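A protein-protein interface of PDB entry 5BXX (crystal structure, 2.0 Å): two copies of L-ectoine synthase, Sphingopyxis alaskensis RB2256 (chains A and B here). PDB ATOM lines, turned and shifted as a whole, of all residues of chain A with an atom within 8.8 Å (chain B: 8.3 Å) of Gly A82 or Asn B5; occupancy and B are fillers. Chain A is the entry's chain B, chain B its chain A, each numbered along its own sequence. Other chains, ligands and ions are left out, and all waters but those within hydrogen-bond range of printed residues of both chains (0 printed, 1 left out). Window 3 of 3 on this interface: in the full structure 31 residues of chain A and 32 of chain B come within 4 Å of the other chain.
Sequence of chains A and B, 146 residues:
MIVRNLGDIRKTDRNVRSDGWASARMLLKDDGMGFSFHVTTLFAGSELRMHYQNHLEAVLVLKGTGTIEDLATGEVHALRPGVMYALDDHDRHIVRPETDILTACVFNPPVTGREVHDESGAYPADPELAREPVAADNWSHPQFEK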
ATOM      1  N   VAL A  59       7.113  25.563   0.915  1.00  0.00           N
ATOM      2  CA  VAL A  59       6.615  25.957   2.229  1.00  0.00           C
ATOM      3  C   VAL A  59       5.124  25.709   2.357  1.00  0.00           C
ATOM      4  O   VAL A  59       4.340  26.151   1.532  1.00  0.00           O
ATOM      5  CB  VAL A  59       6.906  27.430   2.494  1.00  0.00           C
ATOM      6  CG1 VAL A  59       6.300  27.899   3.799  1.00  0.00           C
ATOM      7  CG2 VAL A  59       8.371  27.662   2.486  1.00  0.00           C
ATOM      8  N   LEU A  60       4.723  24.969   3.401  1.00  0.00           N
ATOM      9  CA  LEU A  60       3.312  24.734   3.650  1.00  0.00           C
ATOM     10  C   LEU A  60       2.995  25.459   4.935  1.00  0.00           C
ATOM     11  O   LEU A  60       3.707  25.292   5.937  1.00  0.00           O
ATOM     12  CB  LEU A  60       3.010  23.231   3.745  1.00  0.00           C
ATOM     13  CG  LEU A  60       1.647  22.850   4.282  1.00  0.00           C
ATOM     14  CD1 LEU A  60       0.629  23.081   3.262  1.00  0.00           C
ATOM     15  CD2 LEU A  60       1.594  21.388   4.755  1.00  0.00           C
ATOM     16  N   VAL A  61       1.978  26.313   4.888  1.00  0.00           N
ATOM     17  CA  VAL A  61       1.612  27.089   6.061  1.00  0.00           C
ATOM     18  C   VAL A  61       0.789  26.207   6.977  1.00  0.00           C
ATOM     19  O   VAL A  61      -0.204  25.676   6.548  1.00  0.00           O
ATOM     20  CB  VAL A  61       0.806  28.359   5.688  1.00  0.00           C
ATOM     21  CG1 VAL A  61       0.383  29.131   6.927  1.00  0.00           C
ATOM     22  CG2 VAL A  61       1.649  29.195   4.829  1.00  0.00           C
ATOM     23  N   LEU A  62       1.209  26.072   8.225  1.00  0.00           N
ATOM     24  CA  LEU A  62       0.528  25.171   9.166  1.00  0.00           C
ATOM     25  C   LEU A  62      -0.445  25.920  10.051  1.00  0.00           C
ATOM     26  O   LEU A  62      -1.502  25.420  10.374  1.00  0.00           O
ATOM     27  CB  LEU A  62       1.537  24.466  10.070  1.00  0.00           C
ATOM     28  CG  LEU A  62       2.641  23.699   9.369  1.00  0.00           C
ATOM     29  CD1 LEU A  62       3.397  22.904  10.410  1.00  0.00           C
ATOM     30  CD2 LEU A  62       2.071  22.773   8.364  1.00  0.00           C
ATOM     31  N   LYS A  63      -0.033  27.118  10.452  1.00  0.00           N
ATOM     32  CA  LYS A  63      -0.769  27.947  11.407  1.00  0.00           C
ATOM     33  C   LYS A  63      -0.427  29.425  11.162  1.00  0.00           C
ATOM     34  O   LYS A  63       0.713  29.758  10.873  1.00  0.00           O
ATOM     35  CB  LYS A  63      -0.402  27.583  12.857  1.00  0.00           C
ATOM     36  CG  LYS A  63      -1.590  27.384  13.805  1.00  0.00           C
ATOM     37  CD  LYS A  63      -1.163  27.417  15.310  1.00  0.00           C
ATOM     38  CE  LYS A  63      -1.800  26.316  16.208  1.00  0.00           C
ATOM     39  NZ  LYS A  63      -3.314  26.252  16.232  1.00  0.00           N
ATOM     40  N   GLY A  64      -1.421  30.278  11.290  1.00  0.00           N
ATOM     41  CA  GLY A  64      -1.220  31.725  11.264  1.00  0.00           C
ATOM     42  C   GLY A  64      -1.552  32.323   9.930  1.00  0.00           C
ATOM     43  O   GLY A  64      -1.898  31.609   8.999  1.00  0.00           O
ATOM     44  N   ALA A  78      -2.111  35.790  -0.102  1.00  0.00           N
ATOM     45  CA  ALA A  78      -2.478  35.619   1.279  1.00  0.00           C
ATOM     46  C   ALA A  78      -1.910  34.306   1.778  1.00  0.00           C
ATOM     47  O   ALA A  78      -1.873  33.316   1.043  1.00  0.00           O
ATOM     48  CB  ALA A  78      -3.974  35.627   1.439  1.00  0.00           C
ATOM     49  N   LEU A  79      -1.435  34.336   3.016  1.00  0.00           N
ATOM     50  CA  LEU A  79      -0.972  33.145   3.695  1.00  0.00           C
ATOM     51  C   LEU A  79      -1.978  32.800   4.811  1.00  0.00           C
ATOM     52  O   LEU A  79      -2.312  33.656   5.607  1.00  0.00           O
ATOM     53  CB  LEU A  79       0.418  33.376   4.257  1.00  0.00           C
ATOM     54  CG  LEU A  79       1.557  33.479   3.259  1.00  0.00           C
ATOM     55  CD1 LEU A  79       2.912  33.697   3.915  1.00  0.00           C
ATOM     56  CD2 LEU A  79       1.650  32.293   2.337  1.00  0.00           C
ATOM     57  N   ARG A  80      -2.433  31.540   4.850  1.00  0.00           N
ATOM     58  CA  ARG A  80      -3.348  31.012   5.848  1.00  0.00           C
ATOM     59  C   ARG A  80      -3.042  29.529   5.860  1.00  0.00           C
ATOM     60  O   ARG A  80      -2.454  29.039   4.893  1.00  0.00           O
ATOM     61  CB  ARG A  80      -4.808  31.260   5.492  1.00  0.00           C
ATOM     62  CG  ARG A  80      -5.258  30.699   4.149  1.00  0.00           C
ATOM     63  CD  ARG A  80      -6.741  31.036   3.834  1.00  0.00           C
ATOM     64  NE  ARG A  80      -6.974  32.466   3.694  1.00  0.00           N
ATOM     65  CZ  ARG A  80      -6.862  33.158   2.558  1.00  0.00           C
ATOM     66  NH1 ARG A  80      -6.502  32.570   1.415  1.00  0.00           N
ATOM     67  NH2 ARG A  80      -7.110  34.452   2.572  1.00  0.00           N
ATOM     68  N   PRO A  81      -3.459  28.806   6.920  1.00  0.00           N
ATOM     69  CA  PRO A  81      -3.214  27.356   6.882  1.00  0.00           C
ATOM     70  C   PRO A  81      -3.718  26.689   5.609  1.00  0.00           C
ATOM     71  O   PRO A  81      -4.865  26.857   5.220  1.00  0.00           O
ATOM     72  CB  PRO A  81      -3.986  26.826   8.113  1.00  0.00           C
ATOM     73  CG  PRO A  81      -4.052  27.957   9.024  1.00  0.00           C
ATOM     74  CD  PRO A  81      -4.081  29.211   8.196  1.00  0.00           C
ATOM     75  N   GLY A  82      -2.833  25.930   4.981  1.00  0.00           N
ATOM     76  CA  GLY A  82      -3.195  25.090   3.874  1.00  0.00           C
ATOM     77  C   GLY A  82      -2.695  25.738   2.590  1.00  0.00           C
ATOM     78  O   GLY A  82      -2.750  25.124   1.542  1.00  0.00           O
ATOM     79  N   VAL A  83      -2.174  26.965   2.699  1.00  0.00           N
ATOM     80  CA  VAL A  83      -1.498  27.616   1.589  1.00  0.00           C
ATOM     81  C   VAL A  83      -0.103  27.043   1.443  1.00  0.00           C
ATOM     82  O   VAL A  83       0.654  27.009   2.371  1.00  0.00           O
ATOM     83  CB  VAL A  83      -1.381  29.147   1.780  1.00  0.00           C
ATOM     84  CG1 VAL A  83      -0.513  29.738   0.672  1.00  0.00           C
ATOM     85  CG2 VAL A  83      -2.774  29.802   1.848  1.00  0.00           C
ATOM     86  N   MET A  84       0.236  26.655   0.223  1.00  0.00           N
ATOM     87  CA  MET A  84       1.553  26.138  -0.071  1.00  0.00           C
ATOM     88  C   MET A  84       2.214  27.032  -1.086  1.00  0.00           C
ATOM     89  O   MET A  84       1.623  27.283  -2.135  1.00  0.00           O
ATOM     90  CB  MET A  84       1.442  24.727  -0.622  1.00  0.00           C
ATOM     91  CG  MET A  84       2.745  23.953  -0.656  1.00  0.00           C
ATOM     92  SD  MET A  84       3.835  24.307  -2.006  1.00  0.00           S
ATOM     93  CE  MET A  84       2.767  24.125  -3.449  1.00  0.00           C
ATOM     94  N   TYR A  85       3.401  27.533  -0.790  1.00  0.00           N
ATOM     95  CA  TYR A  85       4.141  28.215  -1.841  1.00  0.00           C
ATOM     96  C   TYR A  85       5.533  27.616  -2.028  1.00  0.00           C
ATOM     97  O   TYR A  85       6.182  27.195  -1.067  1.00  0.00           O
ATOM     98  CB  TYR A  85       4.211  29.710  -1.563  1.00  0.00           C
ATOM     99  CG  TYR A  85       5.001  30.108  -0.349  1.00  0.00           C
ATOM    100  CD1 TYR A  85       6.370  30.289  -0.454  1.00  0.00           C
ATOM    101  CD2 TYR A  85       4.402  30.306   0.873  1.00  0.00           C
ATOM    102  CE1 TYR A  85       7.106  30.665   0.603  1.00  0.00           C
ATOM    103  CE2 TYR A  85       5.139  30.653   1.978  1.00  0.00           C
ATOM    104  CZ  TYR A  85       6.496  30.831   1.834  1.00  0.00           C
ATOM    105  OH  TYR A  85       7.251  31.184   2.911  1.00  0.00           O
ATOM    106  N   LEU A 102       3.453  29.460  11.246  1.00  0.00           N
ATOM    107  CA  LEU A 102       4.183  28.193  11.435  1.00  0.00           C
ATOM    108  C   LEU A 102       4.141  27.521  10.091  1.00  0.00           C
ATOM    109  O   LEU A 102       3.056  27.382   9.501  1.00  0.00           O
ATOM    110  CB  LEU A 102       3.561  27.299  12.525  1.00  0.00           C
ATOM    111  CG  LEU A 102       4.407  26.051  12.846  1.00  0.00           C
ATOM    112  CD1 LEU A 102       5.645  26.364  13.689  1.00  0.00           C
ATOM    113  CD2 LEU A 102       3.538  25.004  13.490  1.00  0.00           C
ATOM    114  N   ILE B   2       5.237  29.346  -7.212  1.00  0.00           N
ATOM    115  CA  ILE B   2       4.000  28.562  -7.279  1.00  0.00           C
ATOM    116  C   ILE B   2       3.248  28.821  -5.980  1.00  0.00           C
ATOM    117  O   ILE B   2       3.849  28.782  -4.891  1.00  0.00           O
ATOM    118  CB  ILE B   2       4.278  27.059  -7.410  1.00  0.00           C
ATOM    119  CG1 ILE B   2       5.263  26.810  -8.556  1.00  0.00           C
ATOM    120  CG2 ILE B   2       2.987  26.262  -7.620  1.00  0.00           C
ATOM    121  CD1 ILE B   2       5.710  25.343  -8.660  1.00  0.00           C
ATOM    122  N   VAL B   3       1.950  29.064  -6.077  1.00  0.00           N
ATOM    123  CA  VAL B   3       1.108  29.219  -4.862  1.00  0.00           C
ATOM    124  C   VAL B   3      -0.112  28.359  -5.073  1.00  0.00           C
ATOM    125  O   VAL B   3      -0.826  28.541  -6.050  1.00  0.00           O
ATOM    126  CB  VAL B   3       0.706  30.676  -4.571  1.00  0.00           C
ATOM    127  CG1 VAL B   3      -0.223  30.766  -3.342  1.00  0.00           C
ATOM    128  CG2 VAL B   3       1.944  31.513  -4.326  1.00  0.00           C
ATOM    129  N   ARG B   4      -0.284  27.361  -4.197  1.00  0.00           N
ATOM    130  CA  ARG B   4      -1.438  26.488  -4.218  1.00  0.00           C
ATOM    131  C   ARG B   4      -2.132  26.510  -2.865  1.00  0.00           C
ATOM    132  O   ARG B   4      -1.630  27.070  -1.878  1.00  0.00           O
ATOM    133  CB  ARG B   4      -1.052  25.057  -4.554  1.00  0.00           C
ATOM    134  CG  ARG B   4      -1.523  24.606  -5.917  1.00  0.00           C
ATOM    135  CD  ARG B   4      -0.484  24.773  -7.013  1.00  0.00           C
ATOM    136  NE  ARG B   4       0.457  23.703  -6.937  1.00  0.00           N
ATOM    137  CZ  ARG B   4       1.282  23.304  -7.904  1.00  0.00           C
ATOM    138  NH1 ARG B   4       1.317  23.838  -9.112  1.00  0.00           N
ATOM    139  NH2 ARG B   4       2.099  22.325  -7.642  1.00  0.00           N
ATOM    140  N   ASN B   5      -3.277  25.850  -2.839  1.00  0.00           N
ATOM    141  CA  ASN B   5      -4.188  25.844  -1.710  1.00  0.00           C
ATOM    142  C   ASN B   5      -4.641  24.414  -1.396  1.00  0.00           C
ATOM    143  O   ASN B   5      -5.254  23.789  -2.257  1.00  0.00           O
ATOM    144  CB  ASN B   5      -5.394  26.715  -2.072  1.00  0.00           C
ATOM    145  CG  ASN B   5      -6.398  26.769  -0.995  1.00  0.00           C
ATOM    146  OD1 ASN B   5      -7.268  25.890  -0.868  1.00  0.00           O
ATOM    147  ND2 ASN B   5      -6.303  27.811  -0.191  1.00  0.00           N
ATOM    148  N   LEU B   6      -4.365  23.889  -0.191  1.00  0.00           N
ATOM    149  CA  LEU B   6      -4.775  22.517   0.167  1.00  0.00           C
ATOM    150  C   LEU B   6      -6.257  22.291  -0.024  1.00  0.00           C
ATOM    151  O   LEU B   6      -6.668  21.279  -0.586  1.00  0.00           O
ATOM    152  CB  LEU B   6      -4.437  22.209   1.641  1.00  0.00           C
ATOM    153  CG  LEU B   6      -4.832  20.794   2.139  1.00  0.00           C
ATOM    154  CD1 LEU B   6      -4.207  19.713   1.353  1.00  0.00           C
ATOM    155  CD2 LEU B   6      -4.293  20.745   3.532  1.00  0.00           C
ATOM    156  N   GLY B   7      -7.061  23.236   0.454  1.00  0.00           N
ATOM    157  CA  GLY B   7      -8.498  23.058   0.433  1.00  0.00           C
ATOM    158  C   GLY B   7      -9.018  22.959  -1.006  1.00  0.00           C
ATOM    159  O   GLY B   7      -9.930  22.181  -1.293  1.00  0.00           O
ATOM    160  N   ASP B   8      -8.459  23.727  -1.938  1.00  0.00           N
ATOM    161  CA  ASP B   8      -8.882  23.552  -3.341  1.00  0.00           C
ATOM    162  C   ASP B   8      -8.400  22.211  -3.895  1.00  0.00           C
ATOM    163  O   ASP B   8      -9.164  21.487  -4.545  1.00  0.00           O
ATOM    164  CB  ASP B   8      -8.382  24.707  -4.237  1.00  0.00           C
ATOM    165  CG  ASP B   8      -8.902  26.058  -3.786  1.00  0.00           C
ATOM    166  OD1 ASP B   8     -10.071  26.124  -3.295  1.00  0.00           O
ATOM    167  OD2 ASP B   8      -8.140  27.045  -3.917  1.00  0.00           O
ATOM    168  N   ILE B   9      -7.151  21.856  -3.623  1.00  0.00           N
ATOM    169  CA  ILE B   9      -6.601  20.587  -4.132  1.00  0.00           C
ATOM    170  C   ILE B   9      -7.390  19.356  -3.622  1.00  0.00           C
ATOM    171  O   ILE B   9      -7.576  18.397  -4.370  1.00  0.00           O
ATOM    172  CB  ILE B   9      -5.095  20.431  -3.767  1.00  0.00           C
ATOM    173  CG1 ILE B   9      -4.257  21.369  -4.634  1.00  0.00           C
ATOM    174  CG2 ILE B   9      -4.588  18.989  -3.983  1.00  0.00           C
ATOM    175  CD1 ILE B   9      -2.915  21.599  -4.087  1.00  0.00           C
ATOM    176  N   ARG B  10      -7.882  19.404  -2.385  1.00  0.00           N
ATOM    177  CA  ARG B  10      -8.631  18.260  -1.823  1.00  0.00           C
ATOM    178  C   ARG B  10      -9.871  17.930  -2.656  1.00  0.00           C
ATOM    179  O   ARG B  10     -10.354  16.791  -2.652  1.00  0.00           O
ATOM    180  CB  ARG B  10      -9.069  18.543  -0.374  1.00  0.00           C
ATOM    181  CG  ARG B  10      -7.938  18.396   0.645  1.00  0.00           C
ATOM    182  CD  ARG B  10      -7.505  16.970   0.787  1.00  0.00           C
ATOM    183  NE  ARG B  10      -6.840  16.828   2.081  1.00  0.00           N
ATOM    184  CZ  ARG B  10      -6.203  15.733   2.486  1.00  0.00           C
ATOM    185  NH1 ARG B  10      -6.056  14.663   1.713  1.00  0.00           N
ATOM    186  NH2 ARG B  10      -5.710  15.730   3.691  1.00  0.00           N
ATOM    187  N   LYS B  11     -10.371  18.941  -3.362  1.00  0.00           N
ATOM    188  CA  LYS B  11     -11.551  18.793  -4.235  1.00  0.00           C
ATOM    189  C   LYS B  11     -11.237  18.218  -5.640  1.00  0.00           C
ATOM    190  O   LYS B  11     -12.148  18.007  -6.446  1.00  0.00           O
ATOM    191  CB  LYS B  11     -12.281  20.160  -4.394  1.00  0.00           C
ATOM    192  CG  LYS B  11     -12.859  20.741  -3.098  1.00  0.00           C
ATOM    193  CD  LYS B  11     -13.437  22.158  -3.210  1.00  0.00           C
ATOM    194  CE  LYS B  11     -14.381  22.560  -2.048  1.00  0.00           C
ATOM    195  NZ  LYS B  11     -13.820  22.593  -0.647  1.00  0.00           N
ATOM    196  N   THR B  12      -9.966  17.969  -5.948  1.00  0.00           N
ATOM    197  CA  THR B  12      -9.598  17.541  -7.300  1.00  0.00           C
ATOM    198  C   THR B  12      -9.031  16.135  -7.368  1.00  0.00           C
ATOM    199  O   THR B  12      -8.823  15.426  -6.331  1.00  0.00           O
ATOM    200  CB  THR B  12      -8.560  18.491  -7.916  1.00  0.00           C
ATOM    201  OG1 THR B  12      -7.328  18.375  -7.208  1.00  0.00           O
ATOM    202  CG2 THR B  12      -9.042  19.960  -7.888  1.00  0.00           C
ATOM    203  N   ARG B  14      -6.110  15.432  -7.824  1.00  0.00           N
ATOM    204  CA  ARG B  14      -4.787  15.432  -7.186  1.00  0.00           C
ATOM    205  C   ARG B  14      -4.877  15.008  -5.695  1.00  0.00           C
ATOM    206  O   ARG B  14      -3.867  14.904  -5.010  1.00  0.00           O
ATOM    207  CB  ARG B  14      -4.129  16.817  -7.311  1.00  0.00           C
ATOM    208  CG  ARG B  14      -3.806  17.190  -8.769  1.00  0.00           C
ATOM    209  CD  ARG B  14      -2.866  18.384  -8.902  1.00  0.00           C
ATOM    210  NE  ARG B  14      -3.436  19.635  -8.379  1.00  0.00           N
ATOM    211  CZ  ARG B  14      -2.887  20.843  -8.553  1.00  0.00           C
ATOM    212  NH1 ARG B  14      -1.753  20.958  -9.247  1.00  0.00           N
ATOM    213  NH2 ARG B  14      -3.451  21.935  -8.023  1.00  0.00           N
ATOM    214  N   ALA B  24      -3.279  14.501  -0.611  1.00  0.00           N
ATOM    215  CA  ALA B  24      -3.232  15.685  -1.478  1.00  0.00           C
ATOM    216  C   ALA B  24      -1.836  15.968  -2.058  1.00  0.00           C
ATOM    217  O   ALA B  24      -0.914  16.283  -1.326  1.00  0.00           O
ATOM    218  CB  ALA B  24      -3.703  16.855  -0.692  1.00  0.00           C
ATOM    219  N   ARG B  25      -1.707  15.894  -3.387  1.00  0.00           N
ATOM    220  CA  ARG B  25      -0.456  16.211  -4.067  1.00  0.00           C
ATOM    221  C   ARG B  25      -0.361  17.710  -4.253  1.00  0.00           C
ATOM    222  O   ARG B  25      -1.043  18.272  -5.127  1.00  0.00           O
ATOM    223  CB  ARG B  25      -0.370  15.535  -5.437  1.00  0.00           C
ATOM    224  CG  ARG B  25      -0.165  14.037  -5.404  1.00  0.00           C
ATOM    225  CD  ARG B  25      -0.821  13.324  -6.591  1.00  0.00           C
ATOM    226  NE  ARG B  25       0.027  12.448  -7.419  1.00  0.00           N
ATOM    227  CZ  ARG B  25       0.267  11.151  -7.198  1.00  0.00           C
ATOM    228  NH1 ARG B  25      -0.159  10.521  -6.083  1.00  0.00           N
ATOM    229  NH2 ARG B  25       1.013  10.484  -8.076  1.00  0.00           N
ATOM    230  N   MET B  26       0.484  18.341  -3.455  1.00  0.00           N
ATOM    231  CA  MET B  26       0.715  19.786  -3.489  1.00  0.00           C
ATOM    232  C   MET B  26       1.774  20.144  -4.489  1.00  0.00           C
ATOM    233  O   MET B  26       1.611  21.096  -5.237  1.00  0.00           O
ATOM    234  CB  MET B  26       1.182  20.321  -2.134  1.00  0.00           C
ATOM    235  CG  MET B  26       0.345  19.970  -0.879  1.00  0.00           C
ATOM    236  SD  MET B  26      -1.258  20.485  -1.127  1.00  0.00           S
ATOM    237  CE  MET B  26      -1.115  22.199  -0.613  1.00  0.00           C
ATOM    238  N   VAL B  39       0.002  16.358   1.511  1.00  0.00           N
ATOM    239  CA  VAL B  39      -0.688  16.412   2.810  1.00  0.00           C
ATOM    240  C   VAL B  39      -1.597  15.183   2.776  1.00  0.00           C
ATOM    241  O   VAL B  39      -2.466  15.078   1.895  1.00  0.00           O
ATOM    242  CB  VAL B  39      -1.491  17.680   3.043  1.00  0.00           C
ATOM    243  CG1 VAL B  39      -2.315  17.590   4.374  1.00  0.00           C
ATOM    244  CG2 VAL B  39      -0.539  18.864   3.049  1.00  0.00           C
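Hydrophobic or aromatic side chains of chain B within 4 Å of the printed part of chain A: Leu B6, Met B26 and Val B39. Along chain B the printed residues that touch a printed residue of chain A span positions 2 to 39. Hydrophobic or aromatic side chains of chain A that line the printed part of chain B: Leu A60, Val A83, Met A84 and Tyr A85. Among the printed residues, no Asp or Glu carboxylate lies within 4 Å of a Lys or Arg side-chain nitrogen of the other chain.
Leu A79 touches none of the printed residues of chain B. Of the printed residues of chain B, Gly A82 touches Asn B5, Leu B6 and Met B26. Of the printed residues of chain B, Met A84 touches Ile B2 (3.8 Å), Val B3 (3.4 Å), Arg B4 (2.8 Å) and Met B26 (3.6 Å). Of the printed residues of chain B, Tyr A85 touches Ile B2 (3.1 Å). Printed residues of chain A within 4 Å of Ile B2: Met A84 (3.8 Å) and Tyr A85 (3.1 Å). Of chain A, only Gly A82 (3.6 Å) comes within 4 Å of Asn B5. No residue of chain A comes within 4 Å of Gly B7. Of the printed residues of chain A, Met B26 touches Gly A82 and Met A84. The nearest residue of chain A that does not touch Asn B5 is Val A83 (4.5 Å).
Among the printed residues, merely in contact across the chains: Tyr A85 with Ile B2 (3.1 Å), Met A84 with Val B3 (3.4 Å), Val A83 with Arg B4 (3.5 Å), Gly A82 with Asn B5 (3.6 Å), Met A84 with Met B26 (3.6 Å), Leu A60 with Val B39 (3.7 Å), Met A84 with Ile B2 (3.8 Å) and Gly A82 with Met B26 (3.98 Å).
The backbone carbonyl oxygen (O) of Met A84 sits at hydrogen-bond distance from the backbone NH (N) of Arg B4. N of Leu B6 sits at hydrogen-bond distance from O of Gly A82.
The backbone NH (N) of Ala B24 sits at hydrogen-bond distance from the backbone carbonyl oxygen (O) of Val B39, 2.7 Å away. The side-chain amide oxygen (OD1) of Asn B5 sits at hydrogen-bond distance from the backbone NH (N) of Gly B7. N of Val A59 is in hydrogen-bond range of O of Tyr A85 (2.7 Å). OD1 of Asn B5 lies within hydrogen-bond range of N of Asp B8, at 2.7 Å. O of Val A61 sits at hydrogen-bond distance from N of Gly A82 (3.1 Å). NH2 of Arg B4 lies within hydrogen-bond range of O of Met B26.
No position is printed for both chains. Of the 10 pairs that touch across the chains among the printed residues, none has its exchanged pair printed and touching as well.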
